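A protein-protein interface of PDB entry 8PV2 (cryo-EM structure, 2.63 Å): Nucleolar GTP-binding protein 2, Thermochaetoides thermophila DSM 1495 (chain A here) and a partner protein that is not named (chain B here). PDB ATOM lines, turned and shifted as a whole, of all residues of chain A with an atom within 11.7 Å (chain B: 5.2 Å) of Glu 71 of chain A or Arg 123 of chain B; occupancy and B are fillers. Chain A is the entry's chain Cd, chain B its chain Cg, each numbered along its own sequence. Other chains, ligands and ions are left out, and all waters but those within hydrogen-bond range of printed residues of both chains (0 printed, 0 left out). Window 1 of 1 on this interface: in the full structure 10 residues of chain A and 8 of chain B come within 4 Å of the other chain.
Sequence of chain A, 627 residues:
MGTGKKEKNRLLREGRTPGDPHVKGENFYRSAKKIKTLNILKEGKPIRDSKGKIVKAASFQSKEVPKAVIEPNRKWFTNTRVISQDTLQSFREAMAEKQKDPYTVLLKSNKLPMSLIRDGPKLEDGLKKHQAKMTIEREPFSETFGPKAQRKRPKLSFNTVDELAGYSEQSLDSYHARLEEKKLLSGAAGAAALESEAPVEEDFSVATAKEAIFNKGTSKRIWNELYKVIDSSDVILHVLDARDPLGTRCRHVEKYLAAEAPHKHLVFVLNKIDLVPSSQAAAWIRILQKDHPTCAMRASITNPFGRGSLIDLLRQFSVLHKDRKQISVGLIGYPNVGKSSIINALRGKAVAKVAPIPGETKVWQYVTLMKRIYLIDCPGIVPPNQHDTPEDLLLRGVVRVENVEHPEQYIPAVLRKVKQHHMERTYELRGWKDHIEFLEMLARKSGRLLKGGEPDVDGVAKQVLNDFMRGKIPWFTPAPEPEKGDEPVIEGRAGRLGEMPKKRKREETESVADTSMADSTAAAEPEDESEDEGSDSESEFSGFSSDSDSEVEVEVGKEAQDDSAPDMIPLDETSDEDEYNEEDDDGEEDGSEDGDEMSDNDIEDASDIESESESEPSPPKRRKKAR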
ATOM      1  N   LYS A  67      10.406  11.683 -12.231  1.00  0.00           N
ATOM      2  CA  LYS A  67      10.966  10.594 -11.442  1.00  0.00           C
ATOM      3  C   LYS A  67      11.961  11.182 -10.452  1.00  0.00           C
ATOM      4  O   LYS A  67      13.053  11.609 -10.838  1.00  0.00           O
ATOM      5  CB  LYS A  67      11.621   9.556 -12.346  1.00  0.00           C
ATOM      6  CG  LYS A  67      10.623   8.667 -13.059  1.00  0.00           C
ATOM      7  CD  LYS A  67       9.691   7.992 -12.067  1.00  0.00           C
ATOM      8  CE  LYS A  67       8.672   7.111 -12.764  1.00  0.00           C
ATOM      9  NZ  LYS A  67       9.309   5.982 -13.484  1.00  0.00           N
ATOM     10  N   ALA A  68      11.584  11.217  -9.179  1.00  0.00           N
ATOM     11  CA  ALA A  68      12.398  11.850  -8.145  1.00  0.00           C
ATOM     12  C   ALA A  68      13.306  10.789  -7.539  1.00  0.00           C
ATOM     13  O   ALA A  68      12.961  10.119  -6.567  1.00  0.00           O
ATOM     14  CB  ALA A  68      11.512  12.513  -7.102  1.00  0.00           C
ATOM     15  N   VAL A  69      14.489  10.640  -8.125  1.00  0.00           N
ATOM     16  CA  VAL A  69      15.431   9.587  -7.773  1.00  0.00           C
ATOM     17  C   VAL A  69      16.799  10.195  -7.493  1.00  0.00           C
ATOM     18  O   VAL A  69      17.216  11.150  -8.158  1.00  0.00           O
ATOM     19  CB  VAL A  69      15.506   8.510  -8.878  1.00  0.00           C
ATOM     20  CG1 VAL A  69      14.196   7.792  -8.995  1.00  0.00           C
ATOM     21  CG2 VAL A  69      15.761   9.166 -10.216  1.00  0.00           C
ATOM     22  N   ILE A  70      17.481   9.662  -6.484  1.00  0.00           N
ATOM     23  CA  ILE A  70      18.828  10.082  -6.114  1.00  0.00           C
ATOM     24  C   ILE A  70      19.776   8.943  -6.455  1.00  0.00           C
ATOM     25  O   ILE A  70      19.591   7.813  -5.989  1.00  0.00           O
ATOM     26  CB  ILE A  70      18.926  10.445  -4.623  1.00  0.00           C
ATOM     27  CG1 ILE A  70      17.988  11.603  -4.275  1.00  0.00           C
ATOM     28  CG2 ILE A  70      20.356  10.785  -4.250  1.00  0.00           C
ATOM     29  CD1 ILE A  70      18.476  12.959  -4.734  1.00  0.00           C
ATOM     30  N   GLU A  71      20.788   9.234  -7.262  1.00  0.00           N
ATOM     31  CA  GLU A  71      21.723   8.189  -7.646  1.00  0.00           C
ATOM     32  C   GLU A  71      22.677   7.864  -6.501  1.00  0.00           C
ATOM     33  O   GLU A  71      22.900   8.689  -5.613  1.00  0.00           O
ATOM     34  CB  GLU A  71      22.515   8.605  -8.885  1.00  0.00           C
ATOM     35  CG  GLU A  71      23.729   9.477  -8.625  1.00  0.00           C
ATOM     36  CD  GLU A  71      23.389  10.949  -8.530  1.00  0.00           C
ATOM     37  OE1 GLU A  71      22.217  11.309  -8.765  1.00  0.00           O
ATOM     38  OE2 GLU A  71      24.295  11.748  -8.218  1.00  0.00           O
ATOM     39  N   PRO A  72      23.212   6.646  -6.470  1.00  0.00           N
ATOM     40  CA  PRO A  72      24.306   6.358  -5.540  1.00  0.00           C
ATOM     41  C   PRO A  72      25.591   7.031  -5.987  1.00  0.00           C
ATOM     42  O   PRO A  72      25.967   6.984  -7.157  1.00  0.00           O
ATOM     43  CB  PRO A  72      24.420   4.830  -5.583  1.00  0.00           C
ATOM     44  CG  PRO A  72      23.764   4.434  -6.841  1.00  0.00           C
ATOM     45  CD  PRO A  72      22.680   5.420  -7.082  1.00  0.00           C
ATOM     46  N   ASN A  73      26.265   7.668  -5.034  1.00  0.00           N
ATOM     47  CA  ASN A  73      27.466   8.434  -5.321  1.00  0.00           C
ATOM     48  C   ASN A  73      28.333   8.441  -4.077  1.00  0.00           C
ATOM     49  O   ASN A  73      27.824   8.568  -2.965  1.00  0.00           O
ATOM     50  CB  ASN A  73      27.123   9.870  -5.735  1.00  0.00           C
ATOM     51  CG  ASN A  73      28.223  10.532  -6.535  1.00  0.00           C
ATOM     52  OD1 ASN A  73      29.406  10.316  -6.291  1.00  0.00           O
ATOM     53  ND2 ASN A  73      27.834  11.362  -7.489  1.00  0.00           N
ATOM     54  N   ARG A  74      29.647   8.323  -4.275  1.00  0.00           N
ATOM     55  CA  ARG A  74      30.566   8.344  -3.145  1.00  0.00           C
ATOM     56  C   ARG A  74      30.658   9.728  -2.522  1.00  0.00           C
ATOM     57  O   ARG A  74      31.098   9.860  -1.376  1.00  0.00           O
ATOM     58  CB  ARG A  74      31.950   7.870  -3.586  1.00  0.00           C
ATOM     59  N   LYS A  75      30.246  10.767  -3.255  1.00  0.00           N
ATOM     60  CA  LYS A  75      30.367  12.132  -2.756  1.00  0.00           C
ATOM     61  C   LYS A  75      29.386  12.426  -1.630  1.00  0.00           C
ATOM     62  O   LYS A  75      29.577  13.389  -0.882  1.00  0.00           O
ATOM     63  CB  LYS A  75      30.163  13.130  -3.897  1.00  0.00           C
ATOM     64  CG  LYS A  75      28.711  13.348  -4.266  1.00  0.00           C
ATOM     65  CD  LYS A  75      28.472  14.710  -4.879  1.00  0.00           C
ATOM     66  CE  LYS A  75      29.013  14.785  -6.284  1.00  0.00           C
ATOM     67  NZ  LYS A  75      28.592  16.040  -6.952  1.00  0.00           N
ATOM     68  N   TRP A  76      28.336  11.613  -1.483  1.00  0.00           N
ATOM     69  CA  TRP A  76      27.375  11.850  -0.413  1.00  0.00           C
ATOM     70  C   TRP A  76      27.926  11.487   0.953  1.00  0.00           C
ATOM     71  O   TRP A  76      27.330  11.862   1.965  1.00  0.00           O
ATOM     72  CB  TRP A  76      26.082  11.062  -0.641  1.00  0.00           C
ATOM     73  CG  TRP A  76      25.415  11.215  -1.980  1.00  0.00           C
ATOM     74  CD1 TRP A  76      24.968  10.205  -2.772  1.00  0.00           C
ATOM     75  CD2 TRP A  76      25.084  12.435  -2.665  1.00  0.00           C
ATOM     76  NE1 TRP A  76      24.398  10.708  -3.910  1.00  0.00           N
ATOM     77  CE2 TRP A  76      24.458  12.073  -3.871  1.00  0.00           C
ATOM     78  CE3 TRP A  76      25.261  13.793  -2.381  1.00  0.00           C
ATOM     79  CZ2 TRP A  76      24.011  13.014  -4.788  1.00  0.00           C
ATOM     80  CZ3 TRP A  76      24.825  14.721  -3.295  1.00  0.00           C
ATOM     81  CH2 TRP A  76      24.203  14.331  -4.483  1.00  0.00           C
ATOM     82  N   PHE A  77      29.043  10.766   1.011  1.00  0.00           N
ATOM     83  CA  PHE A  77      29.545  10.210   2.258  1.00  0.00           C
ATOM     84  C   PHE A  77      30.897  10.789   2.646  1.00  0.00           C
ATOM     85  O   PHE A  77      31.583  10.234   3.506  1.00  0.00           O
ATOM     86  CB  PHE A  77      29.613   8.688   2.149  1.00  0.00           C
ATOM     87  CG  PHE A  77      28.279   8.047   1.903  1.00  0.00           C
ATOM     88  CD1 PHE A  77      27.810   7.863   0.616  1.00  0.00           C
ATOM     89  CD2 PHE A  77      27.487   7.640   2.958  1.00  0.00           C
ATOM     90  CE1 PHE A  77      26.583   7.291   0.391  1.00  0.00           C
ATOM     91  CE2 PHE A  77      26.261   7.060   2.732  1.00  0.00           C
ATOM     92  CZ  PHE A  77      25.810   6.887   1.447  1.00  0.00           C
ATOM     93  N   ARG B 119      28.160  20.945 -14.988  1.00  0.00           N
ATOM     94  CA  ARG B 119      28.788  19.636 -14.867  1.00  0.00           C
ATOM     95  C   ARG B 119      27.806  18.584 -14.374  1.00  0.00           C
ATOM     96  O   ARG B 119      27.946  17.403 -14.702  1.00  0.00           O
ATOM     97  CB  ARG B 119      29.992  19.731 -13.935  1.00  0.00           C
ATOM     98  CG  ARG B 119      31.033  20.729 -14.387  1.00  0.00           C
ATOM     99  CD  ARG B 119      32.169  20.817 -13.397  1.00  0.00           C
ATOM    100  NE  ARG B 119      33.018  19.633 -13.429  1.00  0.00           N
ATOM    101  CZ  ARG B 119      34.149  19.541 -14.112  1.00  0.00           C
ATOM    102  NH1 ARG B 119      34.608  20.551 -14.828  1.00  0.00           N
ATOM    103  NH2 ARG B 119      34.837  18.406 -14.073  1.00  0.00           N
ATOM    104  N   GLU B 120      26.811  18.992 -13.587  1.00  0.00           N
ATOM    105  CA  GLU B 120      25.759  18.069 -13.183  1.00  0.00           C
ATOM    106  C   GLU B 120      24.829  17.753 -14.345  1.00  0.00           C
ATOM    107  O   GLU B 120      24.343  16.624 -14.472  1.00  0.00           O
ATOM    108  CB  GLU B 120      24.980  18.658 -12.009  1.00  0.00           C
ATOM    109  CG  GLU B 120      25.795  18.768 -10.726  1.00  0.00           C
ATOM    110  CD  GLU B 120      26.601  20.056 -10.636  1.00  0.00           C
ATOM    111  OE1 GLU B 120      26.459  20.918 -11.528  1.00  0.00           O
ATOM    112  OE2 GLU B 120      27.386  20.198  -9.674  1.00  0.00           O
ATOM    113  N   GLN B 121      24.567  18.744 -15.196  1.00  0.00           N
ATOM    114  CA  GLN B 121      23.726  18.548 -16.369  1.00  0.00           C
ATOM    115  C   GLN B 121      24.368  17.622 -17.392  1.00  0.00           C
ATOM    116  O   GLN B 121      23.660  16.838 -18.032  1.00  0.00           O
ATOM    117  CB  GLN B 121      23.418  19.908 -16.996  1.00  0.00           C
ATOM    118  CG  GLN B 121      22.642  19.882 -18.288  1.00  0.00           C
ATOM    119  CD  GLN B 121      22.464  21.267 -18.869  1.00  0.00           C
ATOM    120  OE1 GLN B 121      22.886  22.258 -18.277  1.00  0.00           O
ATOM    121  NE2 GLN B 121      21.837  21.343 -20.033  1.00  0.00           N
ATOM    122  N   ARG B 122      25.686  17.678 -17.553  1.00  0.00           N
ATOM    123  CA  ARG B 122      26.363  16.927 -18.602  1.00  0.00           C
ATOM    124  C   ARG B 122      26.924  15.584 -18.132  1.00  0.00           C
ATOM    125  O   ARG B 122      27.823  15.042 -18.782  1.00  0.00           O
ATOM    126  CB  ARG B 122      27.473  17.784 -19.210  1.00  0.00           C
ATOM    127  CG  ARG B 122      28.618  18.060 -18.273  1.00  0.00           C
ATOM    128  CD  ARG B 122      29.421  19.249 -18.706  1.00  0.00           C
ATOM    129  NE  ARG B 122      30.757  19.193 -18.131  1.00  0.00           N
ATOM    130  CZ  ARG B 122      31.622  20.193 -18.157  1.00  0.00           C
ATOM    131  NH1 ARG B 122      31.307  21.362 -18.687  1.00  0.00           N
ATOM    132  NH2 ARG B 122      32.832  20.018 -17.638  1.00  0.00           N
ATOM    133  N   ARG B 123      26.407  15.022 -17.045  1.00  0.00           N
ATOM    134  CA  ARG B 123      26.915  13.749 -16.549  1.00  0.00           C
ATOM    135  C   ARG B 123      26.526  12.595 -17.465  1.00  0.00           C
ATOM    136  O   ARG B 123      25.485  12.616 -18.126  1.00  0.00           O
ATOM    137  CB  ARG B 123      26.395  13.467 -15.143  1.00  0.00           C
ATOM    138  CG  ARG B 123      27.073  14.271 -14.065  1.00  0.00           C
ATOM    139  CD  ARG B 123      26.760  13.711 -12.697  1.00  0.00           C
ATOM    140  NE  ARG B 123      27.183  12.324 -12.568  1.00  0.00           N
ATOM    141  CZ  ARG B 123      26.885  11.544 -11.538  1.00  0.00           C
ATOM    142  NH1 ARG B 123      26.135  11.978 -10.539  1.00  0.00           N
ATOM    143  NH2 ARG B 123      27.350  10.299 -11.511  1.00  0.00           N
ATOM    144  N   ASN B 124      27.383  11.572 -17.492  1.00  0.00           N
ATOM    145  CA  ASN B 124      27.125  10.341 -18.238  1.00  0.00           C
ATOM    146  C   ASN B 124      26.312   9.393 -17.358  1.00  0.00           C
ATOM    147  O   ASN B 124      26.752   8.316 -16.955  1.00  0.00           O
ATOM    148  CB  ASN B 124      28.432   9.702 -18.686  1.00  0.00           C
ATOM    149  CG  ASN B 124      28.221   8.558 -19.655  1.00  0.00           C
ATOM    150  OD1 ASN B 124      27.133   8.376 -20.192  1.00  0.00           O
ATOM    151  ND2 ASN B 124      29.264   7.771 -19.873  1.00  0.00           N
ATOM    152  N   LEU B 125      25.097   9.826 -17.053  1.00  0.00           N
ATOM    153  CA  LEU B 125      24.229   9.058 -16.179  1.00  0.00           C
ATOM    154  C   LEU B 125      22.797   9.483 -16.436  1.00  0.00           C
ATOM    155  O   LEU B 125      22.513  10.673 -16.578  1.00  0.00           O
ATOM    156  CB  LEU B 125      24.584   9.271 -14.705  1.00  0.00           C
ATOM    157  CG  LEU B 125      23.989   8.279 -13.707  1.00  0.00           C
ATOM    158  CD1 LEU B 125      24.472   6.867 -13.981  1.00  0.00           C
ATOM    159  CD2 LEU B 125      24.320   8.697 -12.291  1.00  0.00           C
ATOM    160  N   TRP B 134      19.930   2.907 -13.035  1.00  0.00           N
ATOM    161  CA  TRP B 134      20.750   3.996 -13.543  1.00  0.00           C
ATOM    162  C   TRP B 134      21.657   3.475 -14.646  1.00  0.00           C
ATOM    163  O   TRP B 134      22.278   2.419 -14.507  1.00  0.00           O
ATOM    164  CB  TRP B 134      21.590   4.617 -12.428  1.00  0.00           C
ATOM    165  CG  TRP B 134      20.784   5.379 -11.435  1.00  0.00           C
ATOM    166  CD1 TRP B 134      20.237   4.897 -10.288  1.00  0.00           C
ATOM    167  CD2 TRP B 134      20.425   6.761 -11.502  1.00  0.00           C
ATOM    168  NE1 TRP B 134      19.559   5.891  -9.634  1.00  0.00           N
ATOM    169  CE2 TRP B 134      19.659   7.046 -10.361  1.00  0.00           C
ATOM    170  CE3 TRP B 134      20.680   7.784 -12.416  1.00  0.00           C
ATOM    171  CZ2 TRP B 134      19.145   8.311 -10.109  1.00  0.00           C
ATOM    172  CZ3 TRP B 134      20.169   9.038 -12.164  1.00  0.00           C
ATOM    173  CH2 TRP B 134      19.407   9.291 -11.022  1.00  0.00           C
ATOM    174  N   LYS B 137      24.588   7.290 -20.633  1.00  0.00           N
ATOM    175  CA  LYS B 137      24.038   7.735 -21.906  1.00  0.00           C
ATOM    176  C   LYS B 137      24.876   7.280 -23.093  1.00  0.00           C
ATOM    177  O   LYS B 137      24.356   7.183 -24.208  1.00  0.00           O
ATOM    178  CB  LYS B 137      23.898   9.256 -21.924  1.00  0.00           C
ATOM    179  CG  LYS B 137      23.098   9.823 -20.774  1.00  0.00           C
ATOM    180  CD  LYS B 137      23.148  11.333 -20.792  1.00  0.00           C
ATOM    181  CE  LYS B 137      22.176  11.931 -19.800  1.00  0.00           C
ATOM    182  NZ  LYS B 137      22.316  13.411 -19.728  1.00  0.00           N
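CG2 of Val 69 of chain A touches CZ2 of Trp 134 of chain B, at 3.5 Å.
Ile 70 of chain A touches Trp 134 of chain B.
Glu 71 of chain A touches Leu 125 of chain B (CG to CD2, 3.8 Å).
Trp 134 of chain B touches Glu 71 of chain A (CZ2 to N, 3.4 Å).
Asn 73 of chain A touches Arg 123 of chain B (ND2 to NH1, 3.5 Å).
The guanidinium group (NH1) of Arg 123 of chain B is in salt-bridge range of the side-chain carboxylate (OE2) of Glu 71 of chain A (3.0 Å).
O of Glu 71 of chain A is in hydrogen-bond range of NE1 of Trp 76 of chain A.
The side-chain amide oxygen (OD1) of Asn 73 of chain A lies close to the backbone NH (N) of Lys 75 of chain A, 3.2 Å away.
Of the 11 printed residues of chain A, 4 touch a printed residue of chain B.
Hydrophobic or aromatic side chains of chain A within 4 Å of the printed part of chain B: Val 69.
Hydrophobic or aromatic side chains of chain B that line the printed part of chain A: Leu 125 and Trp 134.
Among the printed residues, Asp or Glu carboxylates within 4 Å of a Lys or Arg side-chain nitrogen of the other chain: Glu 71 of chain A with Arg 123 of chain B (3.0 Å).
Ala 68 of chain A touches none of the printed residues of chain B.
Of the printed residues of chain B, Val 69 of chain A touches Trp 134.
Of the printed residues of chain B, Ile 70 of chain A touches Trp 134 (3.8 Å).
Of the printed residues of chain B, Glu 71 of chain A touches Arg 123, Leu 125 and Trp 134.
Of the printed residues of chain B, Asn 73 of chain A touches Arg 123.
Arg 74 of chain A touches none of the printed residues of chain B.
Arg 123 of chain B touches two residues of chain A.
Leu 125 of chain B touches one residue of chain A.
Of the printed residues of chain A, Trp 134 of chain B touches Val 69, Ile 70 and Glu 71.
The nearest printed residue of chain B that does not touch Glu 71 of chain A is Glu 120 of chain B (7.6 Å).
The nearest residue of chain A that does not touch Arg 123 of chain B is Pro 72 of chain A (5.6 Å).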
